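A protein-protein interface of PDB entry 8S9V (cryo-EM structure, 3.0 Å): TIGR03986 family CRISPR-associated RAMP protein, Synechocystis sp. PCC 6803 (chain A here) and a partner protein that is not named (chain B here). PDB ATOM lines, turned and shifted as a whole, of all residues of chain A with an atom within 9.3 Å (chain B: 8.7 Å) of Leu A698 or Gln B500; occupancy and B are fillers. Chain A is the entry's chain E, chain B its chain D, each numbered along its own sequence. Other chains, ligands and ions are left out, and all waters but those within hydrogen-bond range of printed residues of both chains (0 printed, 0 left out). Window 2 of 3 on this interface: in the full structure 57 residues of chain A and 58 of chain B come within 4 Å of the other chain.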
ATOM      1  N   ARG A 685       3.775   3.967  -7.408  1.00  0.00           N
ATOM      2  CA  ARG A 685       3.481   3.513  -6.059  1.00  0.00           C
ATOM      3  C   ARG A 685       2.188   4.161  -5.617  1.00  0.00           C
ATOM      4  O   ARG A 685       1.940   5.319  -5.928  1.00  0.00           O
ATOM      5  CB  ARG A 685       4.578   3.891  -5.091  1.00  0.00           C
ATOM      6  CG  ARG A 685       5.934   3.839  -5.693  1.00  0.00           C
ATOM      7  CD  ARG A 685       6.954   4.182  -4.679  1.00  0.00           C
ATOM      8  NE  ARG A 685       8.232   4.397  -5.307  1.00  0.00           N
ATOM      9  CZ  ARG A 685       9.341   4.633  -4.637  1.00  0.00           C
ATOM     10  NH1 ARG A 685      10.450   4.941  -5.283  1.00  0.00           N
ATOM     11  NH2 ARG A 685       9.313   4.631  -3.318  1.00  0.00           N
ATOM     12  N   ASP A 692       6.078   5.839   2.725  1.00  0.00           N
ATOM     13  CA  ASP A 692       7.387   5.288   3.033  1.00  0.00           C
ATOM     14  C   ASP A 692       8.502   6.110   2.416  1.00  0.00           C
ATOM     15  O   ASP A 692       9.484   6.444   3.083  1.00  0.00           O
ATOM     16  CB  ASP A 692       7.497   3.862   2.515  1.00  0.00           C
ATOM     17  CG  ASP A 692       6.557   2.926   3.185  1.00  0.00           C
ATOM     18  OD1 ASP A 692       5.970   3.314   4.206  1.00  0.00           O
ATOM     19  OD2 ASP A 692       6.425   1.785   2.706  1.00  0.00           O
ATOM     20  N   TYR A 693       8.374   6.430   1.138  1.00  0.00           N
ATOM     21  CA  TYR A 693       9.395   7.196   0.440  1.00  0.00           C
ATOM     22  C   TYR A 693       9.641   8.555   1.091  1.00  0.00           C
ATOM     23  O   TYR A 693      10.786   8.921   1.372  1.00  0.00           O
ATOM     24  CB  TYR A 693       8.979   7.324  -1.018  1.00  0.00           C
ATOM     25  CG  TYR A 693       9.803   8.223  -1.875  1.00  0.00           C
ATOM     26  CD1 TYR A 693      10.900   7.732  -2.538  1.00  0.00           C
ATOM     27  CD2 TYR A 693       9.472   9.538  -2.057  1.00  0.00           C
ATOM     28  CE1 TYR A 693      11.646   8.521  -3.327  1.00  0.00           C
ATOM     29  CE2 TYR A 693      10.222  10.340  -2.846  1.00  0.00           C
ATOM     30  CZ  TYR A 693      11.306   9.827  -3.485  1.00  0.00           C
ATOM     31  OH  TYR A 693      12.060  10.626  -4.299  1.00  0.00           O
ATOM     32  N   TYR A 694       8.590   9.309   1.367  1.00  0.00           N
ATOM     33  CA  TYR A 694       8.779  10.565   2.075  1.00  0.00           C
ATOM     34  C   TYR A 694       9.063  10.378   3.542  1.00  0.00           C
ATOM     35  O   TYR A 694       9.229  11.376   4.238  1.00  0.00           O
ATOM     36  CB  TYR A 694       7.562  11.466   1.912  1.00  0.00           C
ATOM     37  CG  TYR A 694       7.333  11.843   0.488  1.00  0.00           C
ATOM     38  CD1 TYR A 694       8.285  12.534  -0.222  1.00  0.00           C
ATOM     39  CD2 TYR A 694       6.169  11.499  -0.156  1.00  0.00           C
ATOM     40  CE1 TYR A 694       8.084  12.873  -1.523  1.00  0.00           C
ATOM     41  CE2 TYR A 694       5.964  11.831  -1.465  1.00  0.00           C
ATOM     42  CZ  TYR A 694       6.923  12.518  -2.140  1.00  0.00           C
ATOM     43  OH  TYR A 694       6.740  12.834  -3.456  1.00  0.00           O
ATOM     44  N   GLY A 695       9.061   9.148   4.051  1.00  0.00           N
ATOM     45  CA  GLY A 695       9.391   8.917   5.445  1.00  0.00           C
ATOM     46  C   GLY A 695      10.858   9.041   5.793  1.00  0.00           C
ATOM     47  O   GLY A 695      11.186   9.221   6.966  1.00  0.00           O
ATOM     48  N   SER A 696      11.748   9.001   4.810  1.00  0.00           N
ATOM     49  CA  SER A 696      13.169   8.935   5.104  1.00  0.00           C
ATOM     50  C   SER A 696      13.946   9.649   4.018  1.00  0.00           C
ATOM     51  O   SER A 696      13.568   9.616   2.848  1.00  0.00           O
ATOM     52  CB  SER A 696      13.621   7.484   5.202  1.00  0.00           C
ATOM     53  OG  SER A 696      14.959   7.401   5.612  1.00  0.00           O
ATOM     54  N   LEU A 697      15.058  10.268   4.412  1.00  0.00           N
ATOM     55  CA  LEU A 697      16.010  10.860   3.479  1.00  0.00           C
ATOM     56  C   LEU A 697      17.048   9.889   2.944  1.00  0.00           C
ATOM     57  O   LEU A 697      17.815  10.268   2.057  1.00  0.00           O
ATOM     58  CB  LEU A 697      16.728  12.031   4.132  1.00  0.00           C
ATOM     59  CG  LEU A 697      15.896  13.297   4.157  1.00  0.00           C
ATOM     60  CD1 LEU A 697      14.787  13.144   5.137  1.00  0.00           C
ATOM     61  CD2 LEU A 697      16.737  14.472   4.519  1.00  0.00           C
ATOM     62  N   LEU A 698      17.105   8.670   3.458  1.00  0.00           N
ATOM     63  CA  LEU A 698      17.899   7.610   2.867  1.00  0.00           C
ATOM     64  C   LEU A 698      17.156   6.978   1.700  1.00  0.00           C
ATOM     65  O   LEU A 698      15.940   7.088   1.582  1.00  0.00           O
ATOM     66  CB  LEU A 698      18.236   6.549   3.909  1.00  0.00           C
ATOM     67  CG  LEU A 698      18.884   7.025   5.198  1.00  0.00           C
ATOM     68  CD1 LEU A 698      19.169   5.854   6.086  1.00  0.00           C
ATOM     69  CD2 LEU A 698      20.153   7.722   4.857  1.00  0.00           C
ATOM     70  N   GLU A 699      17.901   6.318   0.821  1.00  0.00           N
ATOM     71  CA  GLU A 699      17.254   5.579  -0.250  1.00  0.00           C
ATOM     72  C   GLU A 699      16.483   4.398   0.316  1.00  0.00           C
ATOM     73  O   GLU A 699      16.984   3.645   1.150  1.00  0.00           O
ATOM     74  CB  GLU A 699      18.262   5.077  -1.276  1.00  0.00           C
ATOM     75  CG  GLU A 699      18.911   6.159  -2.118  1.00  0.00           C
ATOM     76  CD  GLU A 699      19.537   5.608  -3.385  1.00  0.00           C
ATOM     77  OE1 GLU A 699      20.103   4.499  -3.337  1.00  0.00           O
ATOM     78  OE2 GLU A 699      19.451   6.275  -4.436  1.00  0.00           O
ATOM     79  N   THR A 700      15.263   4.230  -0.175  1.00  0.00           N
ATOM     80  CA  THR A 700      14.359   3.177   0.249  1.00  0.00           C
ATOM     81  C   THR A 700      13.720   2.589  -0.999  1.00  0.00           C
ATOM     82  O   THR A 700      13.342   3.326  -1.913  1.00  0.00           O
ATOM     83  CB  THR A 700      13.321   3.733   1.231  1.00  0.00           C
ATOM     84  OG1 THR A 700      12.425   2.697   1.645  1.00  0.00           O
ATOM     85  CG2 THR A 700      12.558   4.867   0.625  1.00  0.00           C
ATOM     86  N   SER A 701      13.615   1.261  -1.040  1.00  0.00           N
ATOM     87  CA  SER A 701      13.358   0.582  -2.304  1.00  0.00           C
ATOM     88  C   SER A 701      11.937   0.801  -2.787  1.00  0.00           C
ATOM     89  O   SER A 701      10.993   0.848  -1.998  1.00  0.00           O
ATOM     90  CB  SER A 701      13.598  -0.915  -2.162  1.00  0.00           C
ATOM     91  OG  SER A 701      12.747  -1.459  -1.173  1.00  0.00           O
ATOM     92  N   LYS B 432      15.347  20.156  12.903  1.00  0.00           N
ATOM     93  CA  LYS B 432      15.539  19.023  12.006  1.00  0.00           C
ATOM     94  C   LYS B 432      14.288  18.601  11.252  1.00  0.00           C
ATOM     95  O   LYS B 432      14.413  18.259  10.065  1.00  0.00           O
ATOM     96  CB  LYS B 432      16.148  17.845  12.760  1.00  0.00           C
ATOM     97  CG  LYS B 432      17.538  18.127  13.239  1.00  0.00           C
ATOM     98  CD  LYS B 432      18.143  16.912  13.874  1.00  0.00           C
ATOM     99  CE  LYS B 432      19.469  17.233  14.490  1.00  0.00           C
ATOM    100  NZ  LYS B 432      20.034  16.043  15.157  1.00  0.00           N
ATOM    101  N   LEU B 440      13.526  17.249   1.525  1.00  0.00           N
ATOM    102  CA  LEU B 440      12.622  16.410   0.741  1.00  0.00           C
ATOM    103  C   LEU B 440      11.980  17.172  -0.407  1.00  0.00           C
ATOM    104  O   LEU B 440      11.748  16.602  -1.474  1.00  0.00           O
ATOM    105  CB  LEU B 440      11.545  15.801   1.629  1.00  0.00           C
ATOM    106  CG  LEU B 440      11.940  14.761   2.654  1.00  0.00           C
ATOM    107  CD1 LEU B 440      10.753  14.481   3.454  1.00  0.00           C
ATOM    108  CD2 LEU B 440      12.374  13.548   1.970  1.00  0.00           C
ATOM    109  N   ARG B 443      14.676  17.396  -3.019  1.00  0.00           N
ATOM    110  CA  ARG B 443      14.802  16.106  -3.697  1.00  0.00           C
ATOM    111  C   ARG B 443      13.804  15.935  -4.831  1.00  0.00           C
ATOM    112  O   ARG B 443      14.128  15.341  -5.858  1.00  0.00           O
ATOM    113  CB  ARG B 443      14.676  14.973  -2.689  1.00  0.00           C
ATOM    114  CG  ARG B 443      14.929  13.628  -3.267  1.00  0.00           C
ATOM    115  CD  ARG B 443      15.006  12.576  -2.198  1.00  0.00           C
ATOM    116  NE  ARG B 443      13.733  12.195  -1.623  1.00  0.00           N
ATOM    117  CZ  ARG B 443      13.630  11.397  -0.573  1.00  0.00           C
ATOM    118  NH1 ARG B 443      12.457  11.030  -0.115  1.00  0.00           N
ATOM    119  NH2 ARG B 443      14.718  10.896  -0.037  1.00  0.00           N
ATOM    120  N   ASN B 490      19.368  12.758  -5.344  1.00  0.00           N
ATOM    121  CA  ASN B 490      18.881  12.045  -4.180  1.00  0.00           C
ATOM    122  C   ASN B 490      19.618  12.414  -2.905  1.00  0.00           C
ATOM    123  O   ASN B 490      19.588  11.647  -1.941  1.00  0.00           O
ATOM    124  CB  ASN B 490      18.981  10.552  -4.441  1.00  0.00           C
ATOM    125  CG  ASN B 490      18.163  10.137  -5.615  1.00  0.00           C
ATOM    126  OD1 ASN B 490      17.393  10.924  -6.140  1.00  0.00           O
ATOM    127  ND2 ASN B 490      18.350   8.913  -6.067  1.00  0.00           N
ATOM    128  N   LEU B 491      20.242  13.583  -2.862  1.00  0.00           N
ATOM    129  CA  LEU B 491      20.941  14.101  -1.692  1.00  0.00           C
ATOM    130  C   LEU B 491      22.121  13.249  -1.253  1.00  0.00           C
ATOM    131  O   LEU B 491      22.666  13.479  -0.180  1.00  0.00           O
ATOM    132  CB  LEU B 491      19.986  14.271  -0.516  1.00  0.00           C
ATOM    133  CG  LEU B 491      18.653  14.921  -0.832  1.00  0.00           C
ATOM    134  CD1 LEU B 491      17.783  14.876   0.395  1.00  0.00           C
ATOM    135  CD2 LEU B 491      18.860  16.341  -1.313  1.00  0.00           C
ATOM    136  N   THR B 492      22.556  12.278  -2.043  1.00  0.00           N
ATOM    137  CA  THR B 492      23.594  11.392  -1.536  1.00  0.00           C
ATOM    138  C   THR B 492      24.907  12.119  -1.286  1.00  0.00           C
ATOM    139  O   THR B 492      25.827  11.519  -0.725  1.00  0.00           O
ATOM    140  CB  THR B 492      23.842  10.225  -2.490  1.00  0.00           C
ATOM    141  OG1 THR B 492      24.408  10.714  -3.704  1.00  0.00           O
ATOM    142  CG2 THR B 492      22.560   9.499  -2.799  1.00  0.00           C
ATOM    143  N   LEU B 494      25.018  14.773   0.733  1.00  0.00           N
ATOM    144  CA  LEU B 494      24.986  14.994   2.174  1.00  0.00           C
ATOM    145  C   LEU B 494      25.398  13.747   2.949  1.00  0.00           C
ATOM    146  O   LEU B 494      25.042  12.623   2.590  1.00  0.00           O
ATOM    147  CB  LEU B 494      23.600  15.436   2.619  1.00  0.00           C
ATOM    148  CG  LEU B 494      23.279  16.864   2.230  1.00  0.00           C
ATOM    149  CD1 LEU B 494      21.836  17.164   2.492  1.00  0.00           C
ATOM    150  CD2 LEU B 494      24.149  17.786   3.015  1.00  0.00           C
ATOM    151  N   ASP B 495      26.166  13.960   4.013  1.00  0.00           N
ATOM    152  CA  ASP B 495      26.743  12.859   4.767  1.00  0.00           C
ATOM    153  C   ASP B 495      25.657  11.909   5.225  1.00  0.00           C
ATOM    154  O   ASP B 495      24.625  12.335   5.741  1.00  0.00           O
ATOM    155  CB  ASP B 495      27.466  13.384   6.001  1.00  0.00           C
ATOM    156  CG  ASP B 495      28.361  14.556   5.700  1.00  0.00           C
ATOM    157  OD1 ASP B 495      28.286  15.082   4.571  1.00  0.00           O
ATOM    158  OD2 ASP B 495      29.140  14.953   6.590  1.00  0.00           O
ATOM    159  N   GLU B 496      25.900  10.610   5.077  1.00  0.00           N
ATOM    160  CA  GLU B 496      24.862   9.655   5.436  1.00  0.00           C
ATOM    161  C   GLU B 496      24.514   9.764   6.909  1.00  0.00           C
ATOM    162  O   GLU B 496      23.350   9.617   7.291  1.00  0.00           O
ATOM    163  CB  GLU B 496      25.273   8.232   5.106  1.00  0.00           C
ATOM    164  CG  GLU B 496      24.140   7.275   5.402  1.00  0.00           C
ATOM    165  CD  GLU B 496      24.299   5.921   4.742  1.00  0.00           C
ATOM    166  OE1 GLU B 496      24.842   5.872   3.617  1.00  0.00           O
ATOM    167  OE2 GLU B 496      23.856   4.910   5.332  1.00  0.00           O
ATOM    168  N   ALA B 497      25.505  10.014   7.756  1.00  0.00           N
ATOM    169  CA  ALA B 497      25.211  10.220   9.164  1.00  0.00           C
ATOM    170  C   ALA B 497      24.328  11.435   9.365  1.00  0.00           C
ATOM    171  O   ALA B 497      23.466  11.442  10.247  1.00  0.00           O
ATOM    172  CB  ALA B 497      26.505  10.372   9.953  1.00  0.00           C
ATOM    173  N   PHE B 498      24.532  12.485   8.575  1.00  0.00           N
ATOM    174  CA  PHE B 498      23.655  13.644   8.681  1.00  0.00           C
ATOM    175  C   PHE B 498      22.277  13.360   8.100  1.00  0.00           C
ATOM    176  O   PHE B 498      21.257  13.661   8.725  1.00  0.00           O
ATOM    177  CB  PHE B 498      24.290  14.844   8.009  1.00  0.00           C
ATOM    178  CG  PHE B 498      23.437  16.051   8.024  1.00  0.00           C
ATOM    179  CD1 PHE B 498      23.122  16.665   9.211  1.00  0.00           C
ATOM    180  CD2 PHE B 498      22.977  16.597   6.857  1.00  0.00           C
ATOM    181  CE1 PHE B 498      22.345  17.790   9.231  1.00  0.00           C
ATOM    182  CE2 PHE B 498      22.204  17.716   6.873  1.00  0.00           C
ATOM    183  CZ  PHE B 498      21.887  18.317   8.062  1.00  0.00           C
ATOM    184  N   ARG B 499      22.217  12.762   6.913  1.00  0.00           N
ATOM    185  CA  ARG B 499      20.922  12.372   6.372  1.00  0.00           C
ATOM    186  C   ARG B 499      20.217  11.373   7.265  1.00  0.00           C
ATOM    187  O   ARG B 499      18.987  11.359   7.325  1.00  0.00           O
ATOM    188  CB  ARG B 499      21.061  11.792   4.972  1.00  0.00           C
ATOM    189  CG  ARG B 499      21.363  12.799   3.920  1.00  0.00           C
ATOM    190  CD  ARG B 499      21.262  12.176   2.568  1.00  0.00           C
ATOM    191  NE  ARG B 499      22.336  11.240   2.307  1.00  0.00           N
ATOM    192  CZ  ARG B 499      22.145   9.979   1.965  1.00  0.00           C
ATOM    193  NH1 ARG B 499      23.176   9.185   1.754  1.00  0.00           N
ATOM    194  NH2 ARG B 499      20.922   9.510   1.847  1.00  0.00           N
ATOM    195  N   GLN B 500      20.961  10.503   7.933  1.00  0.00           N
ATOM    196  CA  GLN B 500      20.320   9.571   8.847  1.00  0.00           C
ATOM    197  C   GLN B 500      19.865  10.246  10.136  1.00  0.00           C
ATOM    198  O   GLN B 500      18.876   9.816  10.733  1.00  0.00           O
ATOM    199  CB  GLN B 500      21.239   8.398   9.106  1.00  0.00           C
ATOM    200  CG  GLN B 500      20.556   7.248   9.758  1.00  0.00           C
ATOM    201  CD  GLN B 500      21.325   5.990   9.514  1.00  0.00           C
ATOM    202  OE1 GLN B 500      22.512   6.033   9.207  1.00  0.00           O
ATOM    203  NE2 GLN B 500      20.653   4.855   9.613  1.00  0.00           N
ATOM    204  N   ASP B 501      20.596  11.250  10.614  1.00  0.00           N
ATOM    205  CA  ASP B 501      20.116  12.049  11.739  1.00  0.00           C
ATOM    206  C   ASP B 501      18.832  12.802  11.427  1.00  0.00           C
ATOM    207  O   ASP B 501      17.886  12.781  12.214  1.00  0.00           O
ATOM    208  CB  ASP B 501      21.172  13.045  12.178  1.00  0.00           C
ATOM    209  CG  ASP B 501      20.701  13.879  13.342  1.00  0.00           C
ATOM    210  OD1 ASP B 501      19.731  13.458  14.002  1.00  0.00           O
ATOM    211  OD2 ASP B 501      21.276  14.960  13.594  1.00  0.00           O
ATOM    212  N   LEU B 502      18.803  13.522  10.311  1.00  0.00           N
ATOM    213  CA  LEU B 502      17.583  14.199   9.884  1.00  0.00           C
ATOM    214  C   LEU B 502      16.427  13.229   9.713  1.00  0.00           C
ATOM    215  O   LEU B 502      15.298  13.528  10.102  1.00  0.00           O
ATOM    216  CB  LEU B 502      17.837  14.945   8.584  1.00  0.00           C
ATOM    217  CG  LEU B 502      18.750  16.156   8.647  1.00  0.00           C
ATOM    218  CD1 LEU B 502      18.817  16.792   7.293  1.00  0.00           C
ATOM    219  CD2 LEU B 502      18.240  17.130   9.661  1.00  0.00           C
ATOM    220  N   SER B 503      16.680  12.070   9.114  1.00  0.00           N
ATOM    221  CA  SER B 503      15.630  11.071   8.981  1.00  0.00           C
ATOM    222  C   SER B 503      15.071  10.657  10.330  1.00  0.00           C
ATOM    223  O   SER B 503      13.875  10.390  10.453  1.00  0.00           O
ATOM    224  CB  SER B 503      16.172   9.844   8.259  1.00  0.00           C
ATOM    225  OG  SER B 503      16.671  10.190   6.988  1.00  0.00           O
ATOM    226  N   THR B 504      15.918  10.574  11.349  1.00  0.00           N
ATOM    227  CA  THR B 504      15.451  10.193  12.675  1.00  0.00           C
ATOM    228  C   THR B 504      14.565  11.259  13.301  1.00  0.00           C
ATOM    229  O   THR B 504      13.493  10.951  13.823  1.00  0.00           O
ATOM    230  CB  THR B 504      16.637   9.887  13.569  1.00  0.00           C
ATOM    231  OG1 THR B 504      17.404   8.845  12.974  1.00  0.00           O
ATOM    232  CG2 THR B 504      16.162   9.421  14.898  1.00  0.00           C
ATOM    233  N   ALA B 505      15.013  12.511  13.312  1.00  0.00           N
ATOM    234  CA  ALA B 505      14.180  13.577  13.858  1.00  0.00           C
ATOM    235  C   ALA B 505      12.897  13.743  13.064  1.00  0.00           C
ATOM    236  O   ALA B 505      11.846  14.044  13.632  1.00  0.00           O
ATOM    237  CB  ALA B 505      14.952  14.886  13.882  1.00  0.00           C
ATOM    238  N   TRP B 506      12.971  13.575  11.746  1.00  0.00           N
ATOM    239  CA  TRP B 506      11.791  13.605  10.888  1.00  0.00           C
ATOM    240  C   TRP B 506      10.820  12.476  11.199  1.00  0.00           C
ATOM    241  O   TRP B 506       9.635  12.712  11.424  1.00  0.00           O
ATOM    242  CB  TRP B 506      12.252  13.531   9.438  1.00  0.00           C
ATOM    243  CG  TRP B 506      11.212  13.481   8.382  1.00  0.00           C
ATOM    244  CD1 TRP B 506      11.022  12.479   7.494  1.00  0.00           C
ATOM    245  CD2 TRP B 506      10.268  14.491   8.051  1.00  0.00           C
ATOM    246  NE1 TRP B 506      10.001  12.784   6.655  1.00  0.00           N
ATOM    247  CE2 TRP B 506       9.527  14.024   6.974  1.00  0.00           C
ATOM    248  CE3 TRP B 506       9.968  15.737   8.574  1.00  0.00           C
ATOM    249  CZ2 TRP B 506       8.515  14.754   6.413  1.00  0.00           C
ATOM    250  CZ3 TRP B 506       8.971  16.453   8.018  1.00  0.00           C
ATOM    251  CH2 TRP B 506       8.248  15.963   6.957  1.00  0.00           C
ATOM    252  N   LYS B 507      11.307  11.244  11.251  1.00  0.00           N
ATOM    253  CA  LYS B 507      10.457  10.122  11.617  1.00  0.00           C
ATOM    254  C   LYS B 507       9.842  10.270  12.998  1.00  0.00           C
ATOM    255  O   LYS B 507       8.704   9.850  13.217  1.00  0.00           O
ATOM    256  CB  LYS B 507      11.259   8.835  11.547  1.00  0.00           C
ATOM    257  CG  LYS B 507      11.465   8.338  10.156  1.00  0.00           C
ATOM    258  CD  LYS B 507      12.229   7.054  10.169  1.00  0.00           C
ATOM    259  CE  LYS B 507      12.215   6.411   8.818  1.00  0.00           C
ATOM    260  NZ  LYS B 507      12.832   5.070   8.863  1.00  0.00           N
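Of chain B, only Arg B499 (3.6 Å), Gln B500 (3.95 Å) and Ser B503 (3.9 Å) come within 4 Å of Leu A698. Printed residues of chain A within 4 Å of Gln B500: Leu A698. Arg B499 touches two residues of chain A. Of chain A, only Ser A696, Leu A697 and Leu A698 come within 4 Å of Ser B503. Printed residues of chain A within 4 Å of Lys B507: Gly A695 (3.3 Å). Of the printed residues of chain A, Arg B443 touches Tyr A693 (3.1 Å), Ser A696 (3.4 Å) and Leu A697 (3.7 Å). Of the printed residues of chain B, Tyr A694 touches Leu B440 and Trp B506. The nearest printed residue of chain A that does not touch Leu B440 is Leu A697 (4.002 Å).
The guanidinium group of Arg B443 sits at hydrogen-bond distance from the backbone carbonyl oxygen of Tyr A693 (3.1 Å). O of Ser A696 sits at hydrogen-bond distance from NH2 of Arg B443, 3.4 Å away. ND2 of Asn B490 sits at hydrogen-bond distance from OE2 of Glu A699 (3.3 Å). The guanidinium group (NH2) of Arg B499 sits at hydrogen-bond distance from the backbone carbonyl oxygen (O) of Leu A697 (3.2 Å). OG of Ser B503 lies within hydrogen-bond range of N of Leu A697 (3.0 Å). The indole nitrogen (NE1) of Trp B506 is in hydrogen-bond range of the backbone carbonyl oxygen (O) of Tyr A694 (2.9 Å).
O of Leu B491 lies close to NE of Arg B499 (3.4 Å). The backbone carbonyl oxygen of Leu B494 is in hydrogen-bond range of the guanidinium group of Arg B499 (3.1 Å). The backbone carbonyl oxygen of Arg B499 lies within hydrogen-bond range of the side-chain hydroxyl of Ser B503, 2.6 Å away. The side-chain hydroxyl (OG1) of Thr B504 is in hydrogen-bond range of the backbone carbonyl oxygen (O) of Gln B500, at 2.9 Å. OG of Ser A696 lies within hydrogen-bond range of N of Leu A698.
Of the 20 printed residues of chain B, 8 touch a printed residue of chain A. Hydrophobic or aromatic side chains of chain B within 4 Å of the printed part of chain A: Leu B440 and Trp B506. Printed residues of chain A that touch a printed residue of chain B: Tyr A693, Tyr A694, Gly A695, Ser A696, Leu A697, Leu A698 and Glu A699. Hydrophobic or aromatic side chains of chain A that line the printed part of chain B: Tyr A693, Leu A697 and Leu A698. Among the printed residues, 14 pairs touch across the chains.
Leu B440 touches Tyr A694. CD1 of Trp B506 touches O of Gly A695 (3.3 Å). Gly A695 touches Lys B507 (O to CG, 3.3 Å). OG of Ser A696 touches OG of Ser B503, at 3.6 Å. Arg B443 touches Leu A697. Leu A698 touches Arg B499 (CD2 to NH2, 3.6 Å). NE2 of Gln B500 touches CD1 of Leu A698, at 3.95 Å. OG of Ser B503 touches N of Leu A698 (3.9 Å).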
